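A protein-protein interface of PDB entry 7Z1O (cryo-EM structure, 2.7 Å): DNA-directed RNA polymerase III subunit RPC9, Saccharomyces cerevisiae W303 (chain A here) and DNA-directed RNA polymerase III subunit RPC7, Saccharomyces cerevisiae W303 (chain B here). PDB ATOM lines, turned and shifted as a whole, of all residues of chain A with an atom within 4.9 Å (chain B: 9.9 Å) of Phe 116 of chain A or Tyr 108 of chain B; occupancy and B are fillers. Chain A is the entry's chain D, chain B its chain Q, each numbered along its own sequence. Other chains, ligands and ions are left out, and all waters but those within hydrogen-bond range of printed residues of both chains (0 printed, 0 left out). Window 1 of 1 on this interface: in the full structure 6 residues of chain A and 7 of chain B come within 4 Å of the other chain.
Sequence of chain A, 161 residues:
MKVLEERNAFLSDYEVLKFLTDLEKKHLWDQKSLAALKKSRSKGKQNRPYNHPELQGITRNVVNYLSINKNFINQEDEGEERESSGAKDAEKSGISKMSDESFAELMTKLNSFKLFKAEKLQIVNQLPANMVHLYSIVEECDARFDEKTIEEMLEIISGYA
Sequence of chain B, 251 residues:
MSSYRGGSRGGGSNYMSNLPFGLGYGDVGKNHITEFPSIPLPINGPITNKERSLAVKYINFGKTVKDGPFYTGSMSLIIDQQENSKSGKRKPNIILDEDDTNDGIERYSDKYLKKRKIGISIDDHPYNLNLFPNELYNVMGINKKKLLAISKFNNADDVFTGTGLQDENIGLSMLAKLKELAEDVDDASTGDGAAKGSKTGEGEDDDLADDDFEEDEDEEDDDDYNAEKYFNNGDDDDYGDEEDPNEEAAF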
ATOM      1  N   LYS A 114      -5.608 -13.170 -10.600  1.00  0.00           N
ATOM      2  CA  LYS A 114      -5.596 -12.008 -11.490  1.00  0.00           C
ATOM      3  C   LYS A 114      -5.638 -10.730 -10.647  1.00  0.00           C
ATOM      4  O   LYS A 114      -6.583  -9.940 -10.687  1.00  0.00           O
ATOM      5  CB  LYS A 114      -6.772 -12.093 -12.457  1.00  0.00           C
ATOM      6  CG  LYS A 114      -6.750 -11.154 -13.653  1.00  0.00           C
ATOM      7  CD  LYS A 114      -5.752 -11.630 -14.696  1.00  0.00           C
ATOM      8  CE  LYS A 114      -5.777 -10.744 -15.929  1.00  0.00           C
ATOM      9  NZ  LYS A 114      -7.086 -10.812 -16.633  1.00  0.00           N
ATOM     10  N   LEU A 115      -4.579 -10.538  -9.861  1.00  0.00           N
ATOM     11  CA  LEU A 115      -4.524  -9.467  -8.873  1.00  0.00           C
ATOM     12  C   LEU A 115      -3.247  -8.650  -9.023  1.00  0.00           C
ATOM     13  O   LEU A 115      -2.258  -9.118  -9.595  1.00  0.00           O
ATOM     14  CB  LEU A 115      -4.609 -10.024  -7.449  1.00  0.00           C
ATOM     15  CG  LEU A 115      -5.873 -10.803  -7.087  1.00  0.00           C
ATOM     16  CD1 LEU A 115      -5.700 -11.498  -5.749  1.00  0.00           C
ATOM     17  CD2 LEU A 115      -7.084  -9.887  -7.063  1.00  0.00           C
ATOM     18  N   PHE A 116      -3.284  -7.424  -8.504  1.00  0.00           N
ATOM     19  CA  PHE A 116      -2.150  -6.513  -8.501  1.00  0.00           C
ATOM     20  C   PHE A 116      -1.402  -6.562  -7.171  1.00  0.00           C
ATOM     21  O   PHE A 116      -1.799  -7.242  -6.224  1.00  0.00           O
ATOM     22  CB  PHE A 116      -2.611  -5.086  -8.796  1.00  0.00           C
ATOM     23  CG  PHE A 116      -2.849  -4.814 -10.249  1.00  0.00           C
ATOM     24  CD1 PHE A 116      -2.273  -5.616 -11.218  1.00  0.00           C
ATOM     25  CD2 PHE A 116      -3.652  -3.759 -10.648  1.00  0.00           C
ATOM     26  CE1 PHE A 116      -2.482  -5.363 -12.557  1.00  0.00           C
ATOM     27  CE2 PHE A 116      -3.869  -3.508 -11.988  1.00  0.00           C
ATOM     28  CZ  PHE A 116      -3.285  -4.310 -12.942  1.00  0.00           C
ATOM     29  N   LYS A 117      -0.292  -5.821  -7.118  1.00  0.00           N
ATOM     30  CA  LYS A 117       0.550  -5.806  -5.926  1.00  0.00           C
ATOM     31  C   LYS A 117      -0.162  -5.148  -4.750  1.00  0.00           C
ATOM     32  O   LYS A 117      -0.080  -5.628  -3.613  1.00  0.00           O
ATOM     33  CB  LYS A 117       1.866  -5.088  -6.230  1.00  0.00           C
ATOM     34  CG  LYS A 117       2.880  -5.130  -5.100  1.00  0.00           C
ATOM     35  CD  LYS A 117       4.120  -4.324  -5.450  1.00  0.00           C
ATOM     36  CE  LYS A 117       4.974  -5.043  -6.480  1.00  0.00           C
ATOM     37  NZ  LYS A 117       6.234  -4.305  -6.767  1.00  0.00           N
ATOM     38  N   ALA A 118      -0.864  -4.041  -5.006  1.00  0.00           N
ATOM     39  CA  ALA A 118      -1.573  -3.340  -3.938  1.00  0.00           C
ATOM     40  C   ALA A 118      -2.702  -4.188  -3.366  1.00  0.00           C
ATOM     41  O   ALA A 118      -2.904  -4.229  -2.145  1.00  0.00           O
ATOM     42  CB  ALA A 118      -2.119  -2.013  -4.459  1.00  0.00           C
ATOM     43  N   GLU A 119      -3.454  -4.864  -4.238  1.00  0.00           N
ATOM     44  CA  GLU A 119      -4.549  -5.713  -3.781  1.00  0.00           C
ATOM     45  C   GLU A 119      -4.030  -6.875  -2.944  1.00  0.00           C
ATOM     46  O   GLU A 119      -4.593  -7.190  -1.888  1.00  0.00           O
ATOM     47  CB  GLU A 119      -5.347  -6.222  -4.983  1.00  0.00           C
ATOM     48  CG  GLU A 119      -5.947  -5.116  -5.837  1.00  0.00           C
ATOM     49  CD  GLU A 119      -6.323  -5.590  -7.227  1.00  0.00           C
ATOM     50  OE1 GLU A 119      -6.048  -6.765  -7.551  1.00  0.00           O
ATOM     51  OE2 GLU A 119      -6.893  -4.789  -7.997  1.00  0.00           O
ATOM     52  N   LYS A 120      -2.945  -7.512  -3.392  1.00  0.00           N
ATOM     53  CA  LYS A 120      -2.349  -8.601  -2.624  1.00  0.00           C
ATOM     54  C   LYS A 120      -1.817  -8.103  -1.286  1.00  0.00           C
ATOM     55  O   LYS A 120      -1.954  -8.785  -0.262  1.00  0.00           O
ATOM     56  CB  LYS A 120      -1.235  -9.266  -3.429  1.00  0.00           C
ATOM     57  CG  LYS A 120      -1.725 -10.095  -4.606  1.00  0.00           C
ATOM     58  CD  LYS A 120      -0.593 -10.899  -5.223  1.00  0.00           C
ATOM     59  CE  LYS A 120       0.304 -10.025  -6.083  1.00  0.00           C
ATOM     60  NZ  LYS A 120      -0.363  -9.624  -7.351  1.00  0.00           N
ATOM     61  N   GLU A 139     -11.446  -3.607  -6.519  1.00  0.00           N
ATOM     62  CA  GLU A 139     -12.508  -2.853  -7.166  1.00  0.00           C
ATOM     63  C   GLU A 139     -12.828  -3.434  -8.541  1.00  0.00           C
ATOM     64  O   GLU A 139     -11.947  -3.943  -9.241  1.00  0.00           O
ATOM     65  CB  GLU A 139     -12.118  -1.372  -7.243  1.00  0.00           C
ATOM     66  CG  GLU A 139     -10.856  -1.048  -8.041  1.00  0.00           C
ATOM     67  CD  GLU A 139     -11.113  -0.870  -9.520  1.00  0.00           C
ATOM     68  OE1 GLU A 139     -12.277  -0.624  -9.889  1.00  0.00           O
ATOM     69  OE2 GLU A 139     -10.154  -0.970 -10.312  1.00  0.00           O
ATOM     70  N   GLU A 140     -14.109  -3.349  -8.913  1.00  0.00           N
ATOM     71  CA  GLU A 140     -14.681  -4.062 -10.062  1.00  0.00           C
ATOM     72  C   GLU A 140     -14.413  -5.563  -9.972  1.00  0.00           C
ATOM     73  O   GLU A 140     -13.843  -6.179 -10.875  1.00  0.00           O
ATOM     74  CB  GLU A 140     -14.189  -3.490 -11.394  1.00  0.00           C
ATOM     75  CG  GLU A 140     -14.532  -2.029 -11.609  1.00  0.00           C
ATOM     76  CD  GLU A 140     -13.997  -1.493 -12.921  1.00  0.00           C
ATOM     77  OE1 GLU A 140     -12.836  -1.802 -13.263  1.00  0.00           O
ATOM     78  OE2 GLU A 140     -14.739  -0.762 -13.611  1.00  0.00           O
ATOM     79  N   ARG A 144     -14.228  -8.566 -13.209  1.00  0.00           N
ATOM     80  CA  ARG A 144     -12.950  -9.251 -13.355  1.00  0.00           C
ATOM     81  C   ARG A 144     -12.996 -10.713 -12.945  1.00  0.00           C
ATOM     82  O   ARG A 144     -12.344 -11.545 -13.579  1.00  0.00           O
ATOM     83  CB  ARG A 144     -11.866  -8.531 -12.538  1.00  0.00           C
ATOM     84  CG  ARG A 144     -10.449  -8.826 -13.002  1.00  0.00           C
ATOM     85  CD  ARG A 144      -9.415  -8.321 -12.006  1.00  0.00           C
ATOM     86  NE  ARG A 144      -9.750  -7.002 -11.482  1.00  0.00           N
ATOM     87  CZ  ARG A 144      -9.102  -6.404 -10.492  1.00  0.00           C
ATOM     88  NH1 ARG A 144      -8.073  -6.979  -9.893  1.00  0.00           N
ATOM     89  NH2 ARG A 144      -9.497  -5.198 -10.093  1.00  0.00           N
ATOM     90  N   GLY B 104       4.091   5.506  -8.178  1.00  0.00           N
ATOM     91  CA  GLY B 104       4.558   4.310  -8.854  1.00  0.00           C
ATOM     92  C   GLY B 104       3.669   3.103  -8.645  1.00  0.00           C
ATOM     93  O   GLY B 104       3.882   2.067  -9.284  1.00  0.00           O
ATOM     94  N   ILE B 105       2.679   3.210  -7.756  1.00  0.00           N
ATOM     95  CA  ILE B 105       1.773   2.098  -7.504  1.00  0.00           C
ATOM     96  C   ILE B 105       0.841   1.921  -8.695  1.00  0.00           C
ATOM     97  O   ILE B 105       0.416   2.895  -9.330  1.00  0.00           O
ATOM     98  CB  ILE B 105       1.012   2.331  -6.186  1.00  0.00           C
ATOM     99  CG1 ILE B 105       0.222   1.088  -5.780  1.00  0.00           C
ATOM    100  CG2 ILE B 105       0.117   3.565  -6.261  1.00  0.00           C
ATOM    101  CD1 ILE B 105      -0.265   1.139  -4.356  1.00  0.00           C
ATOM    102  N   GLU B 106       0.554   0.666  -9.033  1.00  0.00           N
ATOM    103  CA  GLU B 106      -0.288   0.331 -10.173  1.00  0.00           C
ATOM    104  C   GLU B 106      -1.633  -0.186  -9.683  1.00  0.00           C
ATOM    105  O   GLU B 106      -1.689  -1.079  -8.831  1.00  0.00           O
ATOM    106  CB  GLU B 106       0.389  -0.714 -11.060  1.00  0.00           C
ATOM    107  CG  GLU B 106       1.571  -0.182 -11.852  1.00  0.00           C
ATOM    108  CD  GLU B 106       1.258   1.117 -12.564  1.00  0.00           C
ATOM    109  OE1 GLU B 106       0.431   1.099 -13.499  1.00  0.00           O
ATOM    110  OE2 GLU B 106       1.836   2.158 -12.187  1.00  0.00           O
ATOM    111  N   ARG B 107      -2.712   0.373 -10.226  1.00  0.00           N
ATOM    112  CA  ARG B 107      -4.065  -0.030  -9.876  1.00  0.00           C
ATOM    113  C   ARG B 107      -4.833  -0.385 -11.139  1.00  0.00           C
ATOM    114  O   ARG B 107      -4.451  -0.013 -12.251  1.00  0.00           O
ATOM    115  CB  ARG B 107      -4.812   1.073  -9.114  1.00  0.00           C
ATOM    116  CG  ARG B 107      -4.194   1.458  -7.785  1.00  0.00           C
ATOM    117  CD  ARG B 107      -5.000   2.561  -7.120  1.00  0.00           C
ATOM    118  NE  ARG B 107      -4.359   3.054  -5.907  1.00  0.00           N
ATOM    119  CZ  ARG B 107      -3.500   4.064  -5.874  1.00  0.00           C
ATOM    120  NH1 ARG B 107      -3.152   4.711  -6.973  1.00  0.00           N
ATOM    121  NH2 ARG B 107      -2.977   4.432  -4.708  1.00  0.00           N
ATOM    122  N   TYR B 108      -5.933  -1.120 -10.952  1.00  0.00           N
ATOM    123  CA  TYR B 108      -6.813  -1.440 -12.070  1.00  0.00           C
ATOM    124  C   TYR B 108      -7.622  -0.230 -12.522  1.00  0.00           C
ATOM    125  O   TYR B 108      -8.255  -0.278 -13.580  1.00  0.00           O
ATOM    126  CB  TYR B 108      -7.740  -2.598 -11.687  1.00  0.00           C
ATOM    127  CG  TYR B 108      -8.383  -3.306 -12.861  1.00  0.00           C
ATOM    128  CD1 TYR B 108      -7.676  -4.246 -13.601  1.00  0.00           C
ATOM    129  CD2 TYR B 108      -9.702  -3.052 -13.214  1.00  0.00           C
ATOM    130  CE1 TYR B 108      -8.259  -4.900 -14.670  1.00  0.00           C
ATOM    131  CE2 TYR B 108     -10.295  -3.702 -14.282  1.00  0.00           C
ATOM    132  CZ  TYR B 108      -9.569  -4.626 -15.006  1.00  0.00           C
ATOM    133  OH  TYR B 108     -10.152  -5.276 -16.068  1.00  0.00           O
ATOM    134  N   SER B 109      -7.604   0.858 -11.748  1.00  0.00           N
ATOM    135  CA  SER B 109      -8.267   2.087 -12.164  1.00  0.00           C
ATOM    136  C   SER B 109      -7.470   2.847 -13.216  1.00  0.00           C
ATOM    137  O   SER B 109      -7.956   3.864 -13.725  1.00  0.00           O
ATOM    138  CB  SER B 109      -8.515   2.986 -10.951  1.00  0.00           C
ATOM    139  OG  SER B 109      -9.328   4.094 -11.297  1.00  0.00           O
ATOM    140  N   ASP B 110      -6.249   2.397 -13.531  1.00  0.00           N
ATOM    141  CA  ASP B 110      -5.468   3.036 -14.587  1.00  0.00           C
ATOM    142  C   ASP B 110      -6.173   2.931 -15.933  1.00  0.00           C
ATOM    143  O   ASP B 110      -6.235   3.908 -16.687  1.00  0.00           O
ATOM    144  CB  ASP B 110      -4.074   2.415 -14.658  1.00  0.00           C
ATOM    145  CG  ASP B 110      -3.190   2.834 -13.500  1.00  0.00           C
ATOM    146  OD1 ASP B 110      -3.365   3.963 -12.995  1.00  0.00           O
ATOM    147  OD2 ASP B 110      -2.321   2.034 -13.094  1.00  0.00           O
ATOM    148  N   LYS B 111      -6.705   1.756 -16.253  1.00  0.00           N
ATOM    149  CA  LYS B 111      -7.635   1.651 -17.365  1.00  0.00           C
ATOM    150  C   LYS B 111      -8.983   2.227 -16.946  1.00  0.00           C
ATOM    151  O   LYS B 111      -9.319   2.267 -15.759  1.00  0.00           O
ATOM    152  CB  LYS B 111      -7.767   0.199 -17.823  1.00  0.00           C
ATOM    153  CG  LYS B 111      -8.347  -0.749 -16.792  1.00  0.00           C
ATOM    154  CD  LYS B 111      -8.170  -2.196 -17.227  1.00  0.00           C
ATOM    155  CE  LYS B 111      -8.982  -2.512 -18.470  1.00  0.00           C
ATOM    156  NZ  LYS B 111     -10.443  -2.431 -18.216  1.00  0.00           N
ATOM    157  N   TYR B 112      -9.743   2.696 -17.939  1.00  0.00           N
ATOM    158  CA  TYR B 112     -10.926   3.561 -17.845  1.00  0.00           C
ATOM    159  C   TYR B 112     -10.543   4.967 -17.387  1.00  0.00           C
ATOM    160  O   TYR B 112     -11.439   5.769 -17.099  1.00  0.00           O
ATOM    161  CB  TYR B 112     -12.036   3.028 -16.920  1.00  0.00           C
ATOM    162  CG  TYR B 112     -12.441   1.595 -17.176  1.00  0.00           C
ATOM    163  CD1 TYR B 112     -12.585   1.113 -18.471  1.00  0.00           C
ATOM    164  CD2 TYR B 112     -12.688   0.726 -16.121  1.00  0.00           C
ATOM    165  CE1 TYR B 112     -12.960  -0.197 -18.707  1.00  0.00           C
ATOM    166  CE2 TYR B 112     -13.062  -0.583 -16.347  1.00  0.00           C
ATOM    167  CZ  TYR B 112     -13.199  -1.039 -17.641  1.00  0.00           C
ATOM    168  OH  TYR B 112     -13.571  -2.344 -17.871  1.00  0.00           O
ATOM    169  N   LEU B 113      -9.255   5.290 -17.305  1.00  0.00           N
ATOM    170  CA  LEU B 113      -8.788   6.631 -16.984  1.00  0.00           C
ATOM    171  C   LEU B 113      -8.056   7.186 -18.198  1.00  0.00           C
ATOM    172  O   LEU B 113      -7.082   6.588 -18.666  1.00  0.00           O
ATOM    173  CB  LEU B 113      -7.878   6.618 -15.750  1.00  0.00           C
ATOM    174  CG  LEU B 113      -7.482   7.951 -15.106  1.00  0.00           C
ATOM    175  CD1 LEU B 113      -7.442   7.805 -13.595  1.00  0.00           C
ATOM    176  CD2 LEU B 113      -6.134   8.436 -15.619  1.00  0.00           C
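Leu 115 of chain A touches none of the printed residues of chain B.
Of chain B, only Glu 106, Arg 107 and Tyr 108 come within 4 Å of Phe 116 of chain A.
Lys 117 of chain A touches none of the printed residues of chain B.
No residue of chain B comes within 4 Å of Glu 119 of chain A.
Printed residues of chain B within 4 Å of Glu 139 of chain A: Tyr 108 and Ser 109.
Of the printed residues of chain A, Arg 107 of chain B touches Phe 116 (3.4 Å).
Of chain A, only Phe 116, Glu 139, Glu 140 and Arg 144 come within 4 Å of Tyr 108 of chain B.
Printed residues of chain A within 4 Å of Ser 109 of chain B: Glu 139 (3.5 Å).
Leu 113 of chain B touches none of the printed residues of chain A.
The nearest residue of chain B that does not touch Phe 116 of chain A is Ser 109 of chain B (5.8 Å).
The nearest residue of chain A that does not touch Tyr 108 of chain B is Glu 119 of chain A (4.4 Å).
The nearest printed residue of chain A that does not touch Tyr 112 of chain B is Glu 139 of chain A (6.4 Å).
The backbone NH (N) of Ser 109 of chain B sits at hydrogen-bond distance from the side-chain carboxylate (OE2) of Glu 139 of chain A (3.5 Å).
Along chain B the printed residues that touch a printed residue of chain A span positions 105 to 112.
Of the 10 printed residues of chain A, 5 touch a printed residue of chain B.
Hydrophobic or aromatic side chains of chain A that line the printed part of chain B: Phe 116 and Ala 118.
OD2 of Asp 110 of chain B lies within hydrogen-bond range of N of Arg 107 of chain B.
NZ of Lys 111 of chain B sits close to OH of Tyr 112 of chain B.
The backbone carbonyl oxygen of Lys 114 of chain A is in hydrogen-bond range of the guanidinium group of Arg 144 of chain A, 3.4 Å away.
The backbone carbonyl oxygen of Phe 116 of chain A lies within hydrogen-bond range of the side-chain amino group of Lys 120 of chain A (3.0 Å).
OE1 of Glu 119 of chain A lies within salt-bridge range of NH1 of Arg 144 of chain A (3.1 Å).
O of Glu 139 of chain A lies within hydrogen-bond range of NH2 of Arg 144 of chain A (2.9 Å).
Among the printed residues, merely in contact across the chains: Glu 140 of chain A with Tyr 112 of chain B (3.2 Å), Glu 139 of chain A with Tyr 108 of chain B (3.2 Å), Phe 116 of chain A with Tyr 108 of chain B (3.3 Å), Glu 140 of chain A with Tyr 108 of chain B (3.3 Å), Phe 116 of chain A with Arg 107 of chain B (3.4 Å), Arg 144 of chain A with Tyr 108 of chain B (3.5 Å), Ala 118 of chain A with Ile 105 of chain B (3.7 Å) and Phe 116 of chain A with Glu 106 of chain B (3.8 Å).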
